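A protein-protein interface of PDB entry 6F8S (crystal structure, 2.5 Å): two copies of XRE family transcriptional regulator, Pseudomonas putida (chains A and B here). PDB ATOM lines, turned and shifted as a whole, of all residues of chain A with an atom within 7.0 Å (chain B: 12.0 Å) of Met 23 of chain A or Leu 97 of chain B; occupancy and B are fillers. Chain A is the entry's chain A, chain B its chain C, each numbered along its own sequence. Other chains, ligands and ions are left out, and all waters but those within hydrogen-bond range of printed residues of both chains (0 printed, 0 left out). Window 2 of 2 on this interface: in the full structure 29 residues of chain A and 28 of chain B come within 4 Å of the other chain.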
ATOM      1  N   GLU A  18     -28.460 -23.872 -29.478  1.00  0.00           N
ATOM      2  CA  GLU A  18     -27.049 -23.915 -29.828  1.00  0.00           C
ATOM      3  C   GLU A  18     -26.263 -22.732 -29.250  1.00  0.00           C
ATOM      4  O   GLU A  18     -25.033 -22.788 -29.144  1.00  0.00           O
ATOM      5  CB  GLU A  18     -26.898 -23.969 -31.347  1.00  0.00           C
ATOM      6  CG  GLU A  18     -27.643 -25.119 -32.001  1.00  0.00           C
ATOM      7  CD  GLU A  18     -27.195 -26.483 -31.504  1.00  0.00           C
ATOM      8  OE1 GLU A  18     -25.989 -26.656 -31.211  1.00  0.00           O
ATOM      9  OE2 GLU A  18     -28.057 -27.387 -31.401  1.00  0.00           O
ATOM     10  N   PHE A  19     -26.966 -21.661 -28.886  1.00  0.00           N
ATOM     11  CA  PHE A  19     -26.315 -20.526 -28.238  1.00  0.00           C
ATOM     12  C   PHE A  19     -26.779 -20.331 -26.795  1.00  0.00           C
ATOM     13  O   PHE A  19     -25.972 -20.443 -25.863  1.00  0.00           O
ATOM     14  CB  PHE A  19     -26.556 -19.234 -29.029  1.00  0.00           C
ATOM     15  CG  PHE A  19     -25.682 -19.098 -30.223  1.00  0.00           C
ATOM     16  CD1 PHE A  19     -26.114 -19.534 -31.462  1.00  0.00           C
ATOM     17  CD2 PHE A  19     -24.422 -18.541 -30.113  1.00  0.00           C
ATOM     18  CE1 PHE A  19     -25.307 -19.404 -32.587  1.00  0.00           C
ATOM     19  CE2 PHE A  19     -23.608 -18.417 -31.222  1.00  0.00           C
ATOM     20  CZ  PHE A  19     -24.052 -18.850 -32.464  1.00  0.00           C
ATOM     21  N   GLN A  20     -28.069 -20.037 -26.621  1.00  0.00           N
ATOM     22  CA  GLN A  20     -28.594 -19.628 -25.322  1.00  0.00           C
ATOM     23  C   GLN A  20     -28.352 -20.655 -24.219  1.00  0.00           C
ATOM     24  O   GLN A  20     -28.008 -20.286 -23.098  1.00  0.00           O
ATOM     25  CB  GLN A  20     -30.096 -19.336 -25.393  1.00  0.00           C
ATOM     26  CG  GLN A  20     -30.609 -18.708 -24.095  1.00  0.00           C
ATOM     27  CD  GLN A  20     -32.104 -18.505 -24.069  1.00  0.00           C
ATOM     28  OE1 GLN A  20     -32.866 -19.388 -24.459  1.00  0.00           O
ATOM     29  NE2 GLN A  20     -32.535 -17.340 -23.592  1.00  0.00           N
ATOM     30  N   LYS A  21     -28.515 -21.932 -24.537  1.00  0.00           N
ATOM     31  CA  LYS A  21     -28.416 -22.979 -23.524  1.00  0.00           C
ATOM     32  C   LYS A  21     -27.022 -23.060 -22.925  1.00  0.00           C
ATOM     33  O   LYS A  21     -26.868 -23.132 -21.715  1.00  0.00           O
ATOM     34  CB  LYS A  21     -28.807 -24.335 -24.111  1.00  0.00           C
ATOM     35  CG  LYS A  21     -29.823 -25.067 -23.276  1.00  0.00           C
ATOM     36  CD  LYS A  21     -30.093 -26.474 -23.777  1.00  0.00           C
ATOM     37  CE  LYS A  21     -28.821 -27.208 -24.169  1.00  0.00           C
ATOM     38  NZ  LYS A  21     -29.153 -28.607 -24.593  1.00  0.00           N
ATOM     39  N   GLU A  22     -26.007 -23.029 -23.777  1.00  0.00           N
ATOM     40  CA  GLU A  22     -24.634 -23.229 -23.339  1.00  0.00           C
ATOM     41  C   GLU A  22     -24.046 -21.950 -22.765  1.00  0.00           C
ATOM     42  O   GLU A  22     -23.206 -21.994 -21.878  1.00  0.00           O
ATOM     43  CB  GLU A  22     -23.772 -23.734 -24.502  1.00  0.00           C
ATOM     44  CG  GLU A  22     -24.362 -24.926 -25.249  1.00  0.00           C
ATOM     45  CD  GLU A  22     -25.435 -24.541 -26.274  1.00  0.00           C
ATOM     46  OE1 GLU A  22     -26.071 -23.474 -26.134  1.00  0.00           O
ATOM     47  OE2 GLU A  22     -25.644 -25.316 -27.230  1.00  0.00           O
ATOM     48  N   MET A  23     -24.489 -20.808 -23.281  1.00  0.00           N
ATOM     49  CA  MET A  23     -24.007 -19.518 -22.809  1.00  0.00           C
ATOM     50  C   MET A  23     -24.710 -19.118 -21.518  1.00  0.00           C
ATOM     51  O   MET A  23     -24.064 -18.753 -20.530  1.00  0.00           O
ATOM     52  CB  MET A  23     -24.209 -18.454 -23.888  1.00  0.00           C
ATOM     53  CG  MET A  23     -23.254 -18.623 -25.058  1.00  0.00           C
ATOM     54  SD  MET A  23     -23.586 -17.513 -26.424  1.00  0.00           S
ATOM     55  CE  MET A  23     -22.868 -15.975 -25.832  1.00  0.00           C
ATOM     56  N   GLY A  24     -26.037 -19.183 -21.532  1.00  0.00           N
ATOM     57  CA  GLY A  24     -26.815 -18.938 -20.337  1.00  0.00           C
ATOM     58  C   GLY A  24     -27.605 -17.648 -20.320  1.00  0.00           C
ATOM     59  O   GLY A  24     -28.523 -17.523 -19.517  1.00  0.00           O
ATOM     60  N   PHE A  25     -27.260 -16.699 -21.193  1.00  0.00           N
ATOM     61  CA  PHE A  25     -27.908 -15.381 -21.203  1.00  0.00           C
ATOM     62  C   PHE A  25     -29.443 -15.454 -21.233  1.00  0.00           C
ATOM     63  O   PHE A  25     -30.022 -16.401 -21.767  1.00  0.00           O
ATOM     64  CB  PHE A  25     -27.404 -14.544 -22.391  1.00  0.00           C
ATOM     65  CG  PHE A  25     -27.663 -15.163 -23.753  1.00  0.00           C
ATOM     66  CD1 PHE A  25     -28.946 -15.174 -24.310  1.00  0.00           C
ATOM     67  CD2 PHE A  25     -26.618 -15.684 -24.501  1.00  0.00           C
ATOM     68  CE1 PHE A  25     -29.185 -15.732 -25.565  1.00  0.00           C
ATOM     69  CE2 PHE A  25     -26.849 -16.236 -25.767  1.00  0.00           C
ATOM     70  CZ  PHE A  25     -28.135 -16.257 -26.296  1.00  0.00           C
ATOM     71  N   ALA A  29     -30.833 -10.025 -21.902  1.00  0.00           N
ATOM     72  CA  ALA A  29     -29.401  -9.782 -22.105  1.00  0.00           C
ATOM     73  C   ALA A  29     -29.067  -9.794 -23.591  1.00  0.00           C
ATOM     74  O   ALA A  29     -28.345  -8.914 -24.093  1.00  0.00           O
ATOM     75  CB  ALA A  29     -28.563 -10.818 -21.369  1.00  0.00           C
ATOM     76  N   LEU A  30     -29.605 -10.786 -24.296  1.00  0.00           N
ATOM     77  CA  LEU A  30     -29.393 -10.875 -25.734  1.00  0.00           C
ATOM     78  C   LEU A  30     -29.963  -9.626 -26.396  1.00  0.00           C
ATOM     79  O   LEU A  30     -29.276  -8.969 -27.172  1.00  0.00           O
ATOM     80  CB  LEU A  30     -30.028 -12.147 -26.312  1.00  0.00           C
ATOM     81  CG  LEU A  30     -29.870 -12.379 -27.817  1.00  0.00           C
ATOM     82  CD1 LEU A  30     -28.398 -12.340 -28.256  1.00  0.00           C
ATOM     83  CD2 LEU A  30     -30.509 -13.689 -28.224  1.00  0.00           C
ATOM     84  N   ALA A  31     -31.205  -9.295 -26.047  1.00  0.00           N
ATOM     85  CA  ALA A  31     -31.889  -8.113 -26.570  1.00  0.00           C
ATOM     86  C   ALA A  31     -31.083  -6.837 -26.365  1.00  0.00           C
ATOM     87  O   ALA A  31     -30.970  -6.025 -27.297  1.00  0.00           O
ATOM     88  CB  ALA A  31     -33.254  -7.971 -25.931  1.00  0.00           C
ATOM     89  N   ALA A  33     -27.788  -6.573 -25.973  1.00  0.00           N
ATOM     90  CA  ALA A  33     -26.618  -6.694 -26.830  1.00  0.00           C
ATOM     91  C   ALA A  33     -26.919  -6.341 -28.289  1.00  0.00           C
ATOM     92  O   ALA A  33     -26.121  -5.665 -28.941  1.00  0.00           O
ATOM     93  CB  ALA A  33     -26.043  -8.114 -26.739  1.00  0.00           C
ATOM     94  N   LEU A  34     -28.065  -6.789 -28.793  1.00  0.00           N
ATOM     95  CA  LEU A  34     -28.437  -6.551 -30.190  1.00  0.00           C
ATOM     96  C   LEU A  34     -28.952  -5.131 -30.445  1.00  0.00           C
ATOM     97  O   LEU A  34     -28.948  -4.652 -31.588  1.00  0.00           O
ATOM     98  CB  LEU A  34     -29.502  -7.559 -30.624  1.00  0.00           C
ATOM     99  CG  LEU A  34     -29.086  -9.013 -30.409  1.00  0.00           C
ATOM    100  CD1 LEU A  34     -30.306  -9.910 -30.222  1.00  0.00           C
ATOM    101  CD2 LEU A  34     -28.223  -9.480 -31.565  1.00  0.00           C
ATOM    102  N   ILE A  61     -23.253  -9.963 -35.983  1.00  0.00           N
ATOM    103  CA  ILE A  61     -22.242  -9.163 -35.305  1.00  0.00           C
ATOM    104  C   ILE A  61     -22.143  -9.542 -33.822  1.00  0.00           C
ATOM    105  O   ILE A  61     -21.046  -9.612 -33.256  1.00  0.00           O
ATOM    106  CB  ILE A  61     -22.529  -7.652 -35.472  1.00  0.00           C
ATOM    107  CG1 ILE A  61     -22.058  -7.201 -36.863  1.00  0.00           C
ATOM    108  CG2 ILE A  61     -21.845  -6.846 -34.370  1.00  0.00           C
ATOM    109  CD1 ILE A  61     -22.802  -5.982 -37.406  1.00  0.00           C
ATOM    110  N   CYS A  62     -23.285  -9.843 -33.211  1.00  0.00           N
ATOM    111  CA  CYS A  62     -23.311 -10.168 -31.791  1.00  0.00           C
ATOM    112  C   CYS A  62     -22.692 -11.508 -31.471  1.00  0.00           C
ATOM    113  O   CYS A  62     -22.033 -11.652 -30.443  1.00  0.00           O
ATOM    114  CB  CYS A  62     -24.739 -10.158 -31.263  1.00  0.00           C
ATOM    115  SG  CYS A  62     -24.821 -10.557 -29.509  1.00  0.00           S
ATOM    116  N   LEU A  63     -22.925 -12.492 -32.339  1.00  0.00           N
ATOM    117  CA  LEU A  63     -22.612 -13.886 -32.031  1.00  0.00           C
ATOM    118  C   LEU A  63     -21.502 -14.451 -32.907  1.00  0.00           C
ATOM    119  O   LEU A  63     -21.287 -15.655 -32.932  1.00  0.00           O
ATOM    120  CB  LEU A  63     -23.864 -14.744 -32.184  1.00  0.00           C
ATOM    121  CG  LEU A  63     -25.045 -14.451 -31.247  1.00  0.00           C
ATOM    122  CD1 LEU A  63     -26.266 -15.213 -31.730  1.00  0.00           C
ATOM    123  CD2 LEU A  63     -24.737 -14.818 -29.796  1.00  0.00           C
ATOM    124  N   ASP A  64     -20.805 -13.564 -33.613  1.00  0.00           N
ATOM    125  CA  ASP A  64     -19.744 -13.915 -34.559  1.00  0.00           C
ATOM    126  C   ASP A  64     -20.160 -14.966 -35.589  1.00  0.00           C
ATOM    127  O   ASP A  64     -19.525 -16.014 -35.708  1.00  0.00           O
ATOM    128  CB  ASP A  64     -18.477 -14.403 -33.826  1.00  0.00           C
ATOM    129  CG  ASP A  64     -17.244 -14.412 -34.751  1.00  0.00           C
ATOM    130  OD1 ASP A  64     -17.372 -13.923 -35.898  1.00  0.00           O
ATOM    131  OD2 ASP A  64     -16.163 -14.899 -34.347  1.00  0.00           O
ATOM    132  N   ILE B  90     -25.461  -0.218 -37.186  1.00  0.00           N
ATOM    133  CA  ILE B  90     -25.529  -1.452 -36.380  1.00  0.00           C
ATOM    134  C   ILE B  90     -24.168  -1.953 -35.882  1.00  0.00           C
ATOM    135  O   ILE B  90     -24.042  -2.414 -34.743  1.00  0.00           O
ATOM    136  CB  ILE B  90     -26.219  -2.595 -37.177  1.00  0.00           C
ATOM    137  CG1 ILE B  90     -27.724  -2.366 -37.228  1.00  0.00           C
ATOM    138  CG2 ILE B  90     -25.931  -3.949 -36.568  1.00  0.00           C
ATOM    139  CD1 ILE B  90     -28.417  -3.090 -38.361  1.00  0.00           C
ATOM    140  N   ILE B  91     -23.149  -1.853 -36.728  1.00  0.00           N
ATOM    141  CA  ILE B  91     -21.826  -2.359 -36.371  1.00  0.00           C
ATOM    142  C   ILE B  91     -21.195  -1.507 -35.271  1.00  0.00           C
ATOM    143  O   ILE B  91     -20.271  -1.946 -34.597  1.00  0.00           O
ATOM    144  CB  ILE B  91     -20.892  -2.420 -37.592  1.00  0.00           C
ATOM    145  CG1 ILE B  91     -19.659  -3.273 -37.278  1.00  0.00           C
ATOM    146  CG2 ILE B  91     -20.536  -1.003 -38.100  1.00  0.00           C
ATOM    147  CD1 ILE B  91     -18.781  -3.539 -38.479  1.00  0.00           C
ATOM    148  N   SER B  93     -23.147  -0.340 -32.787  1.00  0.00           N
ATOM    149  CA  SER B  93     -24.062  -0.476 -31.652  1.00  0.00           C
ATOM    150  C   SER B  93     -23.927  -1.814 -30.923  1.00  0.00           C
ATOM    151  O   SER B  93     -23.795  -1.864 -29.703  1.00  0.00           O
ATOM    152  CB  SER B  93     -25.506  -0.328 -32.122  1.00  0.00           C
ATOM    153  OG  SER B  93     -25.568   0.545 -33.224  1.00  0.00           O
ATOM    154  N   VAL B  94     -23.983  -2.897 -31.684  1.00  0.00           N
ATOM    155  CA  VAL B  94     -24.160  -4.231 -31.116  1.00  0.00           C
ATOM    156  C   VAL B  94     -23.000  -4.642 -30.201  1.00  0.00           C
ATOM    157  O   VAL B  94     -21.833  -4.460 -30.537  1.00  0.00           O
ATOM    158  CB  VAL B  94     -24.340  -5.259 -32.254  1.00  0.00           C
ATOM    159  CG1 VAL B  94     -24.479  -6.661 -31.712  1.00  0.00           C
ATOM    160  CG2 VAL B  94     -25.541  -4.879 -33.122  1.00  0.00           C
ATOM    161  N   GLN B  95     -23.336  -5.170 -29.030  1.00  0.00           N
ATOM    162  CA  GLN B  95     -22.355  -5.736 -28.112  1.00  0.00           C
ATOM    163  C   GLN B  95     -22.019  -7.174 -28.516  1.00  0.00           C
ATOM    164  O   GLN B  95     -22.931  -7.978 -28.722  1.00  0.00           O
ATOM    165  CB  GLN B  95     -22.890  -5.707 -26.681  1.00  0.00           C
ATOM    166  N   ARG B  96     -20.726  -7.492 -28.631  1.00  0.00           N
ATOM    167  CA  ARG B  96     -20.297  -8.846 -28.984  1.00  0.00           C
ATOM    168  C   ARG B  96     -20.273  -9.778 -27.765  1.00  0.00           C
ATOM    169  O   ARG B  96     -19.578  -9.512 -26.795  1.00  0.00           O
ATOM    170  CB  ARG B  96     -18.913  -8.841 -29.655  1.00  0.00           C
ATOM    171  CG  ARG B  96     -18.367 -10.274 -29.871  1.00  0.00           C
ATOM    172  CD  ARG B  96     -17.505 -10.424 -31.140  1.00  0.00           C
ATOM    173  NE  ARG B  96     -18.267 -10.259 -32.382  1.00  0.00           N
ATOM    174  CZ  ARG B  96     -17.844 -10.638 -33.589  1.00  0.00           C
ATOM    175  NH1 ARG B  96     -16.658 -11.234 -33.740  1.00  0.00           N
ATOM    176  NH2 ARG B  96     -18.624 -10.433 -34.652  1.00  0.00           N
ATOM    177  N   LEU B  97     -21.038 -10.866 -27.835  1.00  0.00           N
ATOM    178  CA  LEU B  97     -21.124 -11.851 -26.748  1.00  0.00           C
ATOM    179  C   LEU B  97     -20.302 -13.109 -27.002  1.00  0.00           C
ATOM    180  O   LEU B  97     -20.087 -13.902 -26.093  1.00  0.00           O
ATOM    181  CB  LEU B  97     -22.575 -12.282 -26.514  1.00  0.00           C
ATOM    182  CG  LEU B  97     -23.556 -11.233 -26.005  1.00  0.00           C
ATOM    183  CD1 LEU B  97     -24.964 -11.809 -26.007  1.00  0.00           C
ATOM    184  CD2 LEU B  97     -23.143 -10.779 -24.623  1.00  0.00           C
ATOM    185  N   VAL B  98     -19.870 -13.300 -28.240  1.00  0.00           N
ATOM    186  CA  VAL B  98     -19.161 -14.511 -28.641  1.00  0.00           C
ATOM    187  C   VAL B  98     -17.802 -14.164 -29.236  1.00  0.00           C
ATOM    188  O   VAL B  98     -17.733 -13.398 -30.183  1.00  0.00           O
ATOM    189  CB  VAL B  98     -19.977 -15.326 -29.684  1.00  0.00           C
ATOM    190  CG1 VAL B  98     -19.142 -16.471 -30.261  1.00  0.00           C
ATOM    191  CG2 VAL B  98     -21.267 -15.850 -29.072  1.00  0.00           C
ATOM    192  N   ALA B  99     -16.724 -14.723 -28.689  1.00  0.00           N
ATOM    193  CA  ALA B  99     -15.391 -14.514 -29.263  1.00  0.00           C
ATOM    194  C   ALA B  99     -15.284 -15.156 -30.644  1.00  0.00           C
ATOM    195  O   ALA B  99     -15.612 -14.541 -31.658  1.00  0.00           O
ATOM    196  CB  ALA B  99     -14.316 -15.073 -28.340  1.00  0.00           C
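O of Ile 61 of chain A lies within hydrogen-bond range of NH2 of Arg 96 of chain B (2.9 Å).
The backbone carbonyl oxygen (O) of Gln 95 of chain B is in hydrogen-bond range of the side-chain sulfur (SG) of Cys 62 of chain A (3.3 Å).
The backbone NH of Leu 97 of chain B lies within hydrogen-bond range of the backbone carbonyl oxygen of Cys 62 of chain A.
The side-chain carboxylate of Asp 64 of chain A sits close to the backbone carbonyl oxygen of Ala 99 of chain B (2.8 Å).
The guanidinium group (NH1) of Arg 96 of chain B is in salt-bridge range of the side-chain carboxylate (OD1) of Asp 64 of chain A, 3.5 Å away.
The backbone carbonyl oxygen (O) of Cys 62 of chain A lies close to the backbone NH (N) of Val 98 of chain B (3.5 Å).
O of Ala 33 of chain A lies within hydrogen-bond range of N of Gln 95 of chain B.
Among the printed residues, merely in contact across the chains: Ala 33 of chain A with Val 94 of chain B (3.3 Å), Met 23 of chain A with Leu 97 of chain B (3.5 Å), Leu 63 of chain A with Val 98 of chain B (3.5 Å), Cys 62 of chain A with Val 94 of chain B (3.5 Å), Cys 62 of chain A with Arg 96 of chain B (3.6 Å), Met 23 of chain A with Val 98 of chain B (3.6 Å), Ile 61 of chain A with Val 94 of chain B (3.6 Å), Leu 34 of chain A with Val 94 of chain B (3.7 Å), Ile 61 of chain A with Ile 90 of chain B (3.8 Å), Asp 64 of chain A with Val 98 of chain B (3.9 Å), Ile 61 of chain A with Ile 91 of chain B (3.9 Å) and Ala 33 of chain A with Leu 97 of chain B (3.9 Å).
Of the printed residues of chain B, Met 23 of chain A touches Leu 97 (3.5 Å) and Val 98 (3.6 Å).
Of chain A, only Met 23, Ala 33 and Cys 62 come within 4 Å of Leu 97 of chain B.
No residue of chain B comes within 4 Å of Phe 19 of chain A.
Gly 24 of chain A touches none of the printed residues of chain B.
No residue of chain B comes within 4 Å of Phe 25 of chain A.
No residue of chain B comes within 4 Å of Ala 29 of chain A.
No residue of chain B comes within 4 Å of Leu 30 of chain A.
Ala 33 of chain A touches just these residues of chain B: Val 94 (3.3 Å), Gln 95 (2.8 Å) and Leu 97 (3.9 Å).
Cys 62 of chain A touches just these residues of chain B: Val 94, Gln 95, Arg 96, Leu 97 and Val 98.
Printed residues of chain A within 4 Å of Ile 91 of chain B: Ile 61.
Of the printed residues of chain A, Ala 99 of chain B touches Asp 64.
Of the printed residues of chain A, Ile 90 of chain B touches Ile 61 (3.8 Å).
Of the printed residues of chain A, Val 94 of chain B touches Ala 33, Leu 34, Ile 61 and Cys 62.
Of the printed residues of chain A, Val 98 of chain B touches Met 23, Cys 62, Leu 63 and Asp 64.
Gln 20 of chain A touches none of the printed residues of chain B.
The nearest residue of chain B that does not touch Met 23 of chain A is Ala 99 of chain B (6.9 Å).
The nearest residue of chain A that does not touch Leu 97 of chain B is Leu 30 of chain A (4.1 Å).
The nearest printed residue of chain A that does not touch Gln 95 of chain B is Leu 34 of chain A (5.0 Å).
Of the 9 printed residues of chain B, 8 touch a printed residue of chain A.
Hydrophobic or aromatic side chains of chain B that line the printed part of chain A: Ile 90, Val 94, Leu 97 and Val 98.
Hydrophobic or aromatic side chains of chain A that line the printed part of chain B: Met 23, Ala 33, Ile 61 and Leu 63.
Among the printed residues, 19 pairs touch across the chains.
Among the printed residues, Asp or Glu carboxylates within 4 Å of a Lys or Arg side-chain nitrogen of the other chain: Asp 64 of chain A with Arg 96 of chain B (3.5 Å).
No position is printed for both chains.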
